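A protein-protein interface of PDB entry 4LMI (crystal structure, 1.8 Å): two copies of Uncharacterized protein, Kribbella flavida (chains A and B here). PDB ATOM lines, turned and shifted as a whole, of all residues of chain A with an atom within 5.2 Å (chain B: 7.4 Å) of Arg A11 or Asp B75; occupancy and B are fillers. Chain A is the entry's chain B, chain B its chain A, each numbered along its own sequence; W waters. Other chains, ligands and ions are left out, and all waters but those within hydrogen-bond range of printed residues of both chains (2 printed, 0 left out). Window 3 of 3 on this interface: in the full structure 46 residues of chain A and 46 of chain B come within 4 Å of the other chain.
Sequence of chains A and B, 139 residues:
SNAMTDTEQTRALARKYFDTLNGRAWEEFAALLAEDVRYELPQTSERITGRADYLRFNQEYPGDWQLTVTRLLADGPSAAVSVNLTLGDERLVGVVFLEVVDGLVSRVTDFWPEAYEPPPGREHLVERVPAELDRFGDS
Ala A74 touches its own counterpart, Ala B74. 7 positions are printed for both chains.
The guanidinium group (NH1) of Arg A11 is in salt-bridge range of the side-chain carboxylate (OD2) of Asp B75 (2.8 Å). The backbone NH (N) of Ala A74 is in hydrogen-bond range of the side-chain carboxylate (OD2) of Asp B75.
N of Leu B73 sits at hydrogen-bond distance from O of Ala B80. O of Ala B79 sits at hydrogen-bond distance from N of Leu B98 (2.8 Å). The side-chain carboxylate (OE1) of Glu A8 is in salt-bridge range of the guanidinium group (NE) of Arg A11 (2.8 Å).
Of the 14 printed residues of chain A, 4 touch a printed residue of chain B. Printed residues of chain A that touch a printed residue of chain B: Arg A11, Leu A72, Leu A73 and Ala A74. Hydrophobic or aromatic side chains of chain A within 4 Å of the printed part of chain B: Leu A73. Of the 15 printed residues of chain B, 5 touch a printed residue of chain A. Hydrophobic or aromatic side chains of chain B that line the printed part of chain A: Ala B80. Among the printed residues, 8 pairs touch across the chains. Among the printed residues, Asp or Glu carboxylates within 4 Å of a Lys or Arg side-chain nitrogen of the other chain: Arg A11 with Asp B75.
Arg A11 touches one residue of chain B. Of the printed residues of chain B, Leu A72 touches Asp B75. Of the printed residues of chain B, Leu A73 touches Asp B75, Ser B78, Ala B79 and Ala B80. Asp B75 touches just these residues of chain A: Arg A11, Leu A72, Leu A73 and Ala A74. Leu B98 touches none of the printed residues of chain A. The nearest residue of chain B that does not touch Arg A11 is Gly B76 (6.2 Å).
Asp B75 touches Leu A72 (OD2 to O, 3.9 Å). Leu A73 touches Asp B75. Ser B78 touches Leu A73 (C to CD2, 3.7 Å). Ala B79 touches Leu A73. CD2 of Leu A73 touches N of Ala B80 (3.6 Å). Ala B74 touches Ala A74 (O to O, 3.8 Å).
Water W2 lies within hydrogen-bond range of O of Ala B74 and O of Ala A74. Water W1 lies within hydrogen-bond range of the backbone carbonyl oxygen (O) of Leu A72 (3.1 Å) and the side-chain carboxylate (OD2) of Asp B75 (3.1 Å).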
ATOM      1  N   ASP A   6      18.850  26.537  -2.474  1.00  0.00           N
ATOM      2  CA  ASP A   6      18.952  25.618  -3.602  1.00  0.00           C
ATOM      3  C   ASP A   6      19.535  24.282  -3.137  1.00  0.00           C
ATOM      4  O   ASP A   6      18.993  23.212  -3.424  1.00  0.00           O
ATOM      5  CB  ASP A   6      19.862  26.245  -4.664  1.00  0.00           C
ATOM      6  CG  ASP A   6      19.706  25.606  -6.025  1.00  0.00           C
ATOM      7  OD1 ASP A   6      18.689  24.922  -6.240  1.00  0.00           O
ATOM      8  OD2 ASP A   6      20.593  25.805  -6.886  1.00  0.00           O
ATOM      9  N   THR A   7      20.635  24.374  -2.393  1.00  0.00           N
ATOM     10  CA  THR A   7      21.380  23.218  -1.876  1.00  0.00           C
ATOM     11  C   THR A   7      20.498  22.301  -1.032  1.00  0.00           C
ATOM     12  O   THR A   7      20.474  21.086  -1.253  1.00  0.00           O
ATOM     13  CB  THR A   7      22.627  23.660  -1.081  1.00  0.00           C
ATOM     14  OG1 THR A   7      23.485  24.414  -1.947  1.00  0.00           O
ATOM     15  CG2 THR A   7      23.402  22.441  -0.521  1.00  0.00           C
ATOM     16  N   GLU A   8      19.748  22.871  -0.091  1.00  0.00           N
ATOM     17  CA  GLU A   8      18.914  22.027   0.764  1.00  0.00           C
ATOM     18  C   GLU A   8      17.728  21.411   0.009  1.00  0.00           C
ATOM     19  O   GLU A   8      17.332  20.272   0.284  1.00  0.00           O
ATOM     20  CB  GLU A   8      18.510  22.744   2.061  1.00  0.00           C
ATOM     21  CG  GLU A   8      19.701  23.076   2.969  1.00  0.00           C
ATOM     22  CD  GLU A   8      20.680  21.915   3.156  1.00  0.00           C
ATOM     23  OE1 GLU A   8      20.243  20.806   3.528  1.00  0.00           O
ATOM     24  OE2 GLU A   8      21.900  22.116   2.935  1.00  0.00           O
ATOM     25  N   GLN A   9      17.201  22.147  -0.973  1.00  0.00           N
ATOM     26  CA  GLN A   9      16.162  21.618  -1.860  1.00  0.00           C
ATOM     27  C   GLN A   9      16.678  20.403  -2.635  1.00  0.00           C
ATOM     28  O   GLN A   9      16.017  19.362  -2.699  1.00  0.00           O
ATOM     29  CB  GLN A   9      15.672  22.707  -2.817  1.00  0.00           C
ATOM     30  CG  GLN A   9      14.592  22.250  -3.786  1.00  0.00           C
ATOM     31  CD  GLN A   9      13.798  23.400  -4.377  1.00  0.00           C
ATOM     32  OE1 GLN A   9      14.107  24.573  -4.147  1.00  0.00           O
ATOM     33  NE2 GLN A   9      12.760  23.068  -5.137  1.00  0.00           N
ATOM     34  N   THR A  10      17.872  20.540  -3.201  1.00  0.00           N
ATOM     35  CA  THR A  10      18.529  19.445  -3.913  1.00  0.00           C
ATOM     36  C   THR A  10      18.779  18.246  -3.002  1.00  0.00           C
ATOM     37  O   THR A  10      18.540  17.095  -3.401  1.00  0.00           O
ATOM     38  CB  THR A  10      19.847  19.941  -4.529  1.00  0.00           C
ATOM     39  OG1 THR A  10      19.532  20.905  -5.539  1.00  0.00           O
ATOM     40  CG2 THR A  10      20.653  18.797  -5.154  1.00  0.00           C
ATOM     41  N   ARG A  11      19.251  18.508  -1.782  1.00  0.00           N
ATOM     42  CA  ARG A  11      19.483  17.426  -0.821  1.00  0.00           C
ATOM     43  C   ARG A  11      18.212  16.602  -0.581  1.00  0.00           C
ATOM     44  O   ARG A  11      18.240  15.371  -0.664  1.00  0.00           O
ATOM     45  CB  ARG A  11      20.027  17.959   0.510  1.00  0.00           C
ATOM     46  CG  ARG A  11      20.612  16.868   1.403  1.00  0.00           C
ATOM     47  CD  ARG A  11      21.017  17.374   2.785  1.00  0.00           C
ATOM     48  NE  ARG A  11      21.819  18.596   2.712  1.00  0.00           N
ATOM     49  CZ  ARG A  11      23.117  18.635   2.419  1.00  0.00           C
ATOM     50  NH1 ARG A  11      23.784  17.510   2.185  1.00  0.00           N
ATOM     51  NH2 ARG A  11      23.753  19.803   2.363  1.00  0.00           N
ATOM     52  N   ALA A  12      17.106  17.288  -0.295  1.00  0.00           N
ATOM     53  CA  ALA A  12      15.822  16.634  -0.048  1.00  0.00           C
ATOM     54  C   ALA A  12      15.360  15.864  -1.283  1.00  0.00           C
ATOM     55  O   ALA A  12      14.853  14.739  -1.166  1.00  0.00           O
ATOM     56  CB  ALA A  12      14.769  17.658   0.376  1.00  0.00           C
ATOM     57  N   LEU A  13      15.559  16.454  -2.464  1.00  0.00           N
ATOM     58  CA  LEU A  13      15.116  15.820  -3.696  1.00  0.00           C
ATOM     59  C   LEU A  13      15.934  14.563  -4.026  1.00  0.00           C
ATOM     60  O   LEU A  13      15.361  13.544  -4.421  1.00  0.00           O
ATOM     61  CB  LEU A  13      15.114  16.815  -4.865  1.00  0.00           C
ATOM     62  CG  LEU A  13      14.548  16.306  -6.199  1.00  0.00           C
ATOM     63  CD1 LEU A  13      13.071  15.950  -6.085  1.00  0.00           C
ATOM     64  CD2 LEU A  13      14.756  17.337  -7.296  1.00  0.00           C
ATOM     65  N   ALA A  14      17.254  14.636  -3.853  1.00  0.00           N
ATOM     66  CA  ALA A  14      18.138  13.473  -4.065  1.00  0.00           C
ATOM     67  C   ALA A  14      17.772  12.321  -3.136  1.00  0.00           C
ATOM     68  O   ALA A  14      17.772  11.157  -3.549  1.00  0.00           O
ATOM     69  CB  ALA A  14      19.597  13.857  -3.870  1.00  0.00           C
ATOM     70  N   ARG A  15      17.468  12.645  -1.878  1.00  0.00           N
ATOM     71  CA  ARG A  15      17.041  11.625  -0.920  1.00  0.00           C
ATOM     72  C   ARG A  15      15.754  10.941  -1.397  1.00  0.00           C
ATOM     73  O   ARG A  15      15.663   9.707  -1.385  1.00  0.00           O
ATOM     74  CB  ARG A  15      16.884  12.219   0.495  1.00  0.00           C
ATOM     75  CG  ARG A  15      16.456  11.212   1.557  1.00  0.00           C
ATOM     76  CD  ARG A  15      17.506  10.129   1.792  1.00  0.00           C
ATOM     77  NE  ARG A  15      18.724  10.672   2.398  1.00  0.00           N
ATOM     78  CZ  ARG A  15      19.807   9.960   2.701  1.00  0.00           C
ATOM     79  NH1 ARG A  15      19.843   8.654   2.456  1.00  0.00           N
ATOM     80  NH2 ARG A  15      20.856  10.562   3.249  1.00  0.00           N
ATOM     81  N   LYS A  16      14.778  11.745  -1.823  1.00  0.00           N
ATOM     82  CA  LYS A  16      13.497  11.235  -2.321  1.00  0.00           C
ATOM     83  C   LYS A  16      13.651  10.389  -3.584  1.00  0.00           C
ATOM     84  O   LYS A  16      12.949   9.388  -3.756  1.00  0.00           O
ATOM     85  CB  LYS A  16      12.518  12.384  -2.572  1.00  0.00           C
ATOM     86  CG  LYS A  16      11.926  12.975  -1.307  1.00  0.00           C
ATOM     87  CD  LYS A  16      10.712  13.841  -1.607  1.00  0.00           C
ATOM     88  CE  LYS A  16      10.237  14.580  -0.365  1.00  0.00           C
ATOM     89  NZ  LYS A  16      11.231  15.585   0.106  1.00  0.00           N
ATOM     90  N   LEU A  72      25.746  11.163   0.488  1.00  0.00           N
ATOM     91  CA  LEU A  72      24.874  12.063  -0.254  1.00  0.00           C
ATOM     92  C   LEU A  72      25.370  13.498  -0.109  1.00  0.00           C
ATOM     93  O   LEU A  72      25.262  14.100   0.961  1.00  0.00           O
ATOM     94  CB  LEU A  72      23.414  11.923   0.205  1.00  0.00           C
ATOM     95  CG  LEU A  72      22.309  12.451  -0.727  1.00  0.00           C
ATOM     96  CD1 LEU A  72      20.963  11.839  -0.372  1.00  0.00           C
ATOM     97  CD2 LEU A  72      22.211  13.976  -0.719  1.00  0.00           C
ATOM     98  N   LEU A  73      25.925  14.038  -1.192  1.00  0.00           N
ATOM     99  CA  LEU A  73      26.383  15.424  -1.209  1.00  0.00           C
ATOM    100  C   LEU A  73      25.459  16.270  -2.067  1.00  0.00           C
ATOM    101  O   LEU A  73      25.035  15.832  -3.137  1.00  0.00           O
ATOM    102  CB  LEU A  73      27.818  15.520  -1.737  1.00  0.00           C
ATOM    103  CG  LEU A  73      28.960  15.031  -0.840  1.00  0.00           C
ATOM    104  CD1 LEU A  73      28.996  13.511  -0.728  1.00  0.00           C
ATOM    105  CD2 LEU A  73      30.281  15.550  -1.391  1.00  0.00           C
ATOM    106  N   ALA A  74      25.141  17.469  -1.584  1.00  0.00           N
ATOM    107  CA  ALA A  74      24.347  18.444  -2.338  1.00  0.00           C
ATOM    108  C   ALA A  74      25.106  19.765  -2.405  1.00  0.00           C
ATOM    109  O   ALA A  74      25.707  20.194  -1.419  1.00  0.00           O
ATOM    110  CB  ALA A  74      22.986  18.649  -1.682  1.00  0.00           C
ATOM    111  N   THR B   5      29.523  27.648   7.355  1.00  0.00           N
ATOM    112  CA  THR B   5      29.799  26.343   6.738  1.00  0.00           C
ATOM    113  C   THR B   5      31.238  26.250   6.208  1.00  0.00           C
ATOM    114  O   THR B   5      31.892  27.268   5.956  1.00  0.00           O
ATOM    115  CB  THR B   5      28.812  25.998   5.595  1.00  0.00           C
ATOM    116  OG1 THR B   5      28.984  26.915   4.507  1.00  0.00           O
ATOM    117  CG2 THR B   5      27.360  26.037   6.081  1.00  0.00           C
ATOM    118  N   ASP B   6      31.716  25.019   6.053  1.00  0.00           N
ATOM    119  CA  ASP B   6      33.038  24.757   5.499  1.00  0.00           C
ATOM    120  C   ASP B   6      33.010  24.681   3.959  1.00  0.00           C
ATOM    121  O   ASP B   6      34.055  24.511   3.333  1.00  0.00           O
ATOM    122  CB  ASP B   6      33.607  23.453   6.084  1.00  0.00           C
ATOM    123  CG  ASP B   6      34.191  23.626   7.482  1.00  0.00           C
ATOM    124  OD1 ASP B   6      34.069  24.722   8.071  1.00  0.00           O
ATOM    125  OD2 ASP B   6      34.782  22.650   7.997  1.00  0.00           O
ATOM    126  N   THR B   7      31.825  24.838   3.356  1.00  0.00           N
ATOM    127  CA  THR B   7      31.616  24.492   1.936  1.00  0.00           C
ATOM    128  C   THR B   7      32.596  25.157   0.961  1.00  0.00           C
ATOM    129  O   THR B   7      33.238  24.477   0.161  1.00  0.00           O
ATOM    130  CB  THR B   7      30.163  24.774   1.481  1.00  0.00           C
ATOM    131  OG1 THR B   7      29.259  23.959   2.238  1.00  0.00           O
ATOM    132  CG2 THR B   7      29.974  24.471  -0.025  1.00  0.00           C
ATOM    133  N   GLU B   8      32.703  26.480   1.014  1.00  0.00           N
ATOM    134  CA  GLU B   8      33.560  27.186   0.067  1.00  0.00           C
ATOM    135  C   GLU B   8      35.038  26.928   0.318  1.00  0.00           C
ATOM    136  O   GLU B   8      35.832  26.919  -0.624  1.00  0.00           O
ATOM    137  CB  GLU B   8      33.240  28.689   0.030  1.00  0.00           C
ATOM    138  CG  GLU B   8      31.821  28.999  -0.464  1.00  0.00           C
ATOM    139  CD  GLU B   8      31.450  28.266  -1.754  1.00  0.00           C
ATOM    140  OE1 GLU B   8      32.230  28.320  -2.730  1.00  0.00           O
ATOM    141  OE2 GLU B   8      30.367  27.638  -1.803  1.00  0.00           O
ATOM    142  N   THR B  10      36.115  23.991   1.458  1.00  0.00           N
ATOM    143  CA  THR B  10      36.222  22.663   0.835  1.00  0.00           C
ATOM    144  C   THR B  10      36.320  22.747  -0.696  1.00  0.00           C
ATOM    145  O   THR B  10      37.123  22.042  -1.303  1.00  0.00           O
ATOM    146  CB  THR B  10      35.046  21.764   1.254  1.00  0.00           C
ATOM    147  OG1 THR B  10      35.115  21.536   2.667  1.00  0.00           O
ATOM    148  CG2 THR B  10      35.063  20.413   0.516  1.00  0.00           C
ATOM    149  N   ARG B  11      35.509  23.609  -1.311  1.00  0.00           N
ATOM    150  CA  ARG B  11      35.561  23.793  -2.769  1.00  0.00           C
ATOM    151  C   ARG B  11      36.966  24.189  -3.237  1.00  0.00           C
ATOM    152  O   ARG B  11      37.513  23.585  -4.171  1.00  0.00           O
ATOM    153  CB  ARG B  11      34.530  24.822  -3.243  1.00  0.00           C
ATOM    154  CG  ARG B  11      34.312  24.813  -4.755  1.00  0.00           C
ATOM    155  CD  ARG B  11      33.426  25.970  -5.212  1.00  0.00           C
ATOM    156  NE  ARG B  11      32.202  26.068  -4.407  1.00  0.00           N
ATOM    157  CZ  ARG B  11      31.144  25.260  -4.522  1.00  0.00           C
ATOM    158  NH1 ARG B  11      31.118  24.278  -5.424  1.00  0.00           N
ATOM    159  NH2 ARG B  11      30.097  25.437  -3.729  1.00  0.00           N
ATOM    160  N   LEU B  73      31.716  19.028  -6.657  1.00  0.00           N
ATOM    161  CA  LEU B  73      30.701  19.380  -5.668  1.00  0.00           C
ATOM    162  C   LEU B  73      31.342  19.492  -4.300  1.00  0.00           C
ATOM    163  O   LEU B  73      32.113  18.621  -3.909  1.00  0.00           O
ATOM    164  CB  LEU B  73      29.591  18.325  -5.610  1.00  0.00           C
ATOM    165  CG  LEU B  73      28.613  18.185  -6.774  1.00  0.00           C
ATOM    166  CD1 LEU B  73      29.248  17.475  -7.962  1.00  0.00           C
ATOM    167  CD2 LEU B  73      27.401  17.409  -6.292  1.00  0.00           C
ATOM    168  N   ALA B  74      31.017  20.572  -3.587  1.00  0.00           N
ATOM    169  CA  ALA B  74      31.455  20.780  -2.207  1.00  0.00           C
ATOM    170  C   ALA B  74      30.223  20.884  -1.316  1.00  0.00           C
ATOM    171  O   ALA B  74      29.238  21.525  -1.685  1.00  0.00           O
ATOM    172  CB  ALA B  74      32.305  22.043  -2.096  1.00  0.00           C
ATOM    173  N   ASP B  75      30.283  20.257  -0.147  1.00  0.00           N
ATOM    174  CA  ASP B  75      29.137  20.185   0.760  1.00  0.00           C
ATOM    175  C   ASP B  75      29.679  20.080   2.183  1.00  0.00           C
ATOM    176  O   ASP B  75      30.047  18.997   2.628  1.00  0.00           O
ATOM    177  CB  ASP B  75      28.281  18.961   0.401  1.00  0.00           C
ATOM    178  CG  ASP B  75      27.017  18.829   1.250  1.00  0.00           C
ATOM    179  OD1 ASP B  75      26.733  19.696   2.108  1.00  0.00           O
ATOM    180  OD2 ASP B  75      26.290  17.834   1.045  1.00  0.00           O
ATOM    181  N   GLY B  76      29.738  21.209   2.890  1.00  0.00           N
ATOM    182  CA  GLY B  76      30.381  21.237   4.200  1.00  0.00           C
ATOM    183  C   GLY B  76      31.817  20.747   4.067  1.00  0.00           C
ATOM    184  O   GLY B  76      32.564  21.248   3.221  1.00  0.00           O
ATOM    185  N   PRO B  77      32.198  19.733   4.865  1.00  0.00           N
ATOM    186  CA  PRO B  77      33.556  19.205   4.851  1.00  0.00           C
ATOM    187  C   PRO B  77      33.779  18.081   3.826  1.00  0.00           C
ATOM    188  O   PRO B  77      34.791  17.384   3.903  1.00  0.00           O
ATOM    189  CB  PRO B  77      33.712  18.664   6.273  1.00  0.00           C
ATOM    190  CG  PRO B  77      32.342  18.177   6.617  1.00  0.00           C
ATOM    191  CD  PRO B  77      31.363  19.052   5.875  1.00  0.00           C
ATOM    192  N   SER B  78      32.855  17.916   2.876  1.00  0.00           N
ATOM    193  CA  SER B  78      32.937  16.821   1.895  1.00  0.00           C
ATOM    194  C   SER B  78      32.956  17.334   0.463  1.00  0.00           C
ATOM    195  O   SER B  78      32.333  18.353   0.152  1.00  0.00           O
ATOM    196  CB  SER B  78      31.757  15.851   2.047  1.00  0.00           C
ATOM    197  OG  SER B  78      31.624  15.371   3.372  1.00  0.00           O
ATOM    198  N   ALA B  79      33.660  16.618  -0.412  1.00  0.00           N
ATOM    199  CA  ALA B  79      33.629  16.920  -1.844  1.00  0.00           C
ATOM    200  C   ALA B  79      33.478  15.659  -2.696  1.00  0.00           C
ATOM    201  O   ALA B  79      33.897  14.565  -2.298  1.00  0.00           O
ATOM    202  CB  ALA B  79      34.869  17.712  -2.262  1.00  0.00           C
ATOM    203  N   ALA B  80      32.844  15.817  -3.856  1.00  0.00           N
ATOM    204  CA  ALA B  80      32.767  14.750  -4.846  1.00  0.00           C
ATOM    205  C   ALA B  80      33.229  15.343  -6.159  1.00  0.00           C
ATOM    206  O   ALA B  80      32.715  16.383  -6.596  1.00  0.00           O
ATOM    207  CB  ALA B  80      31.350  14.207  -4.962  1.00  0.00           C
ATOM    208  N   LEU B  98      36.175  13.283  -1.269  1.00  0.00           N
ATOM    209  CA  LEU B  98      37.146  13.817  -0.320  1.00  0.00           C
ATOM    210  C   LEU B  98      36.455  14.175   0.981  1.00  0.00           C
ATOM    211  O   LEU B  98      35.304  14.639   0.975  1.00  0.00           O
ATOM    212  CB  LEU B  98      37.845  15.063  -0.882  1.00  0.00           C
ATOM    213  CG  LEU B  98      38.565  14.997  -2.233  1.00  0.00           C
ATOM    214  CD1 LEU B  98      39.075  16.376  -2.615  1.00  0.00           C
ATOM    215  CD2 LEU B  98      39.703  13.993  -2.229  1.00  0.00           C
HETATM  216  O   HOH W   1      27.294  15.452   2.809  1.00  0.00           O
HETATM  217  O   HOH W   2      26.996  22.460  -0.633  1.00  0.00           O
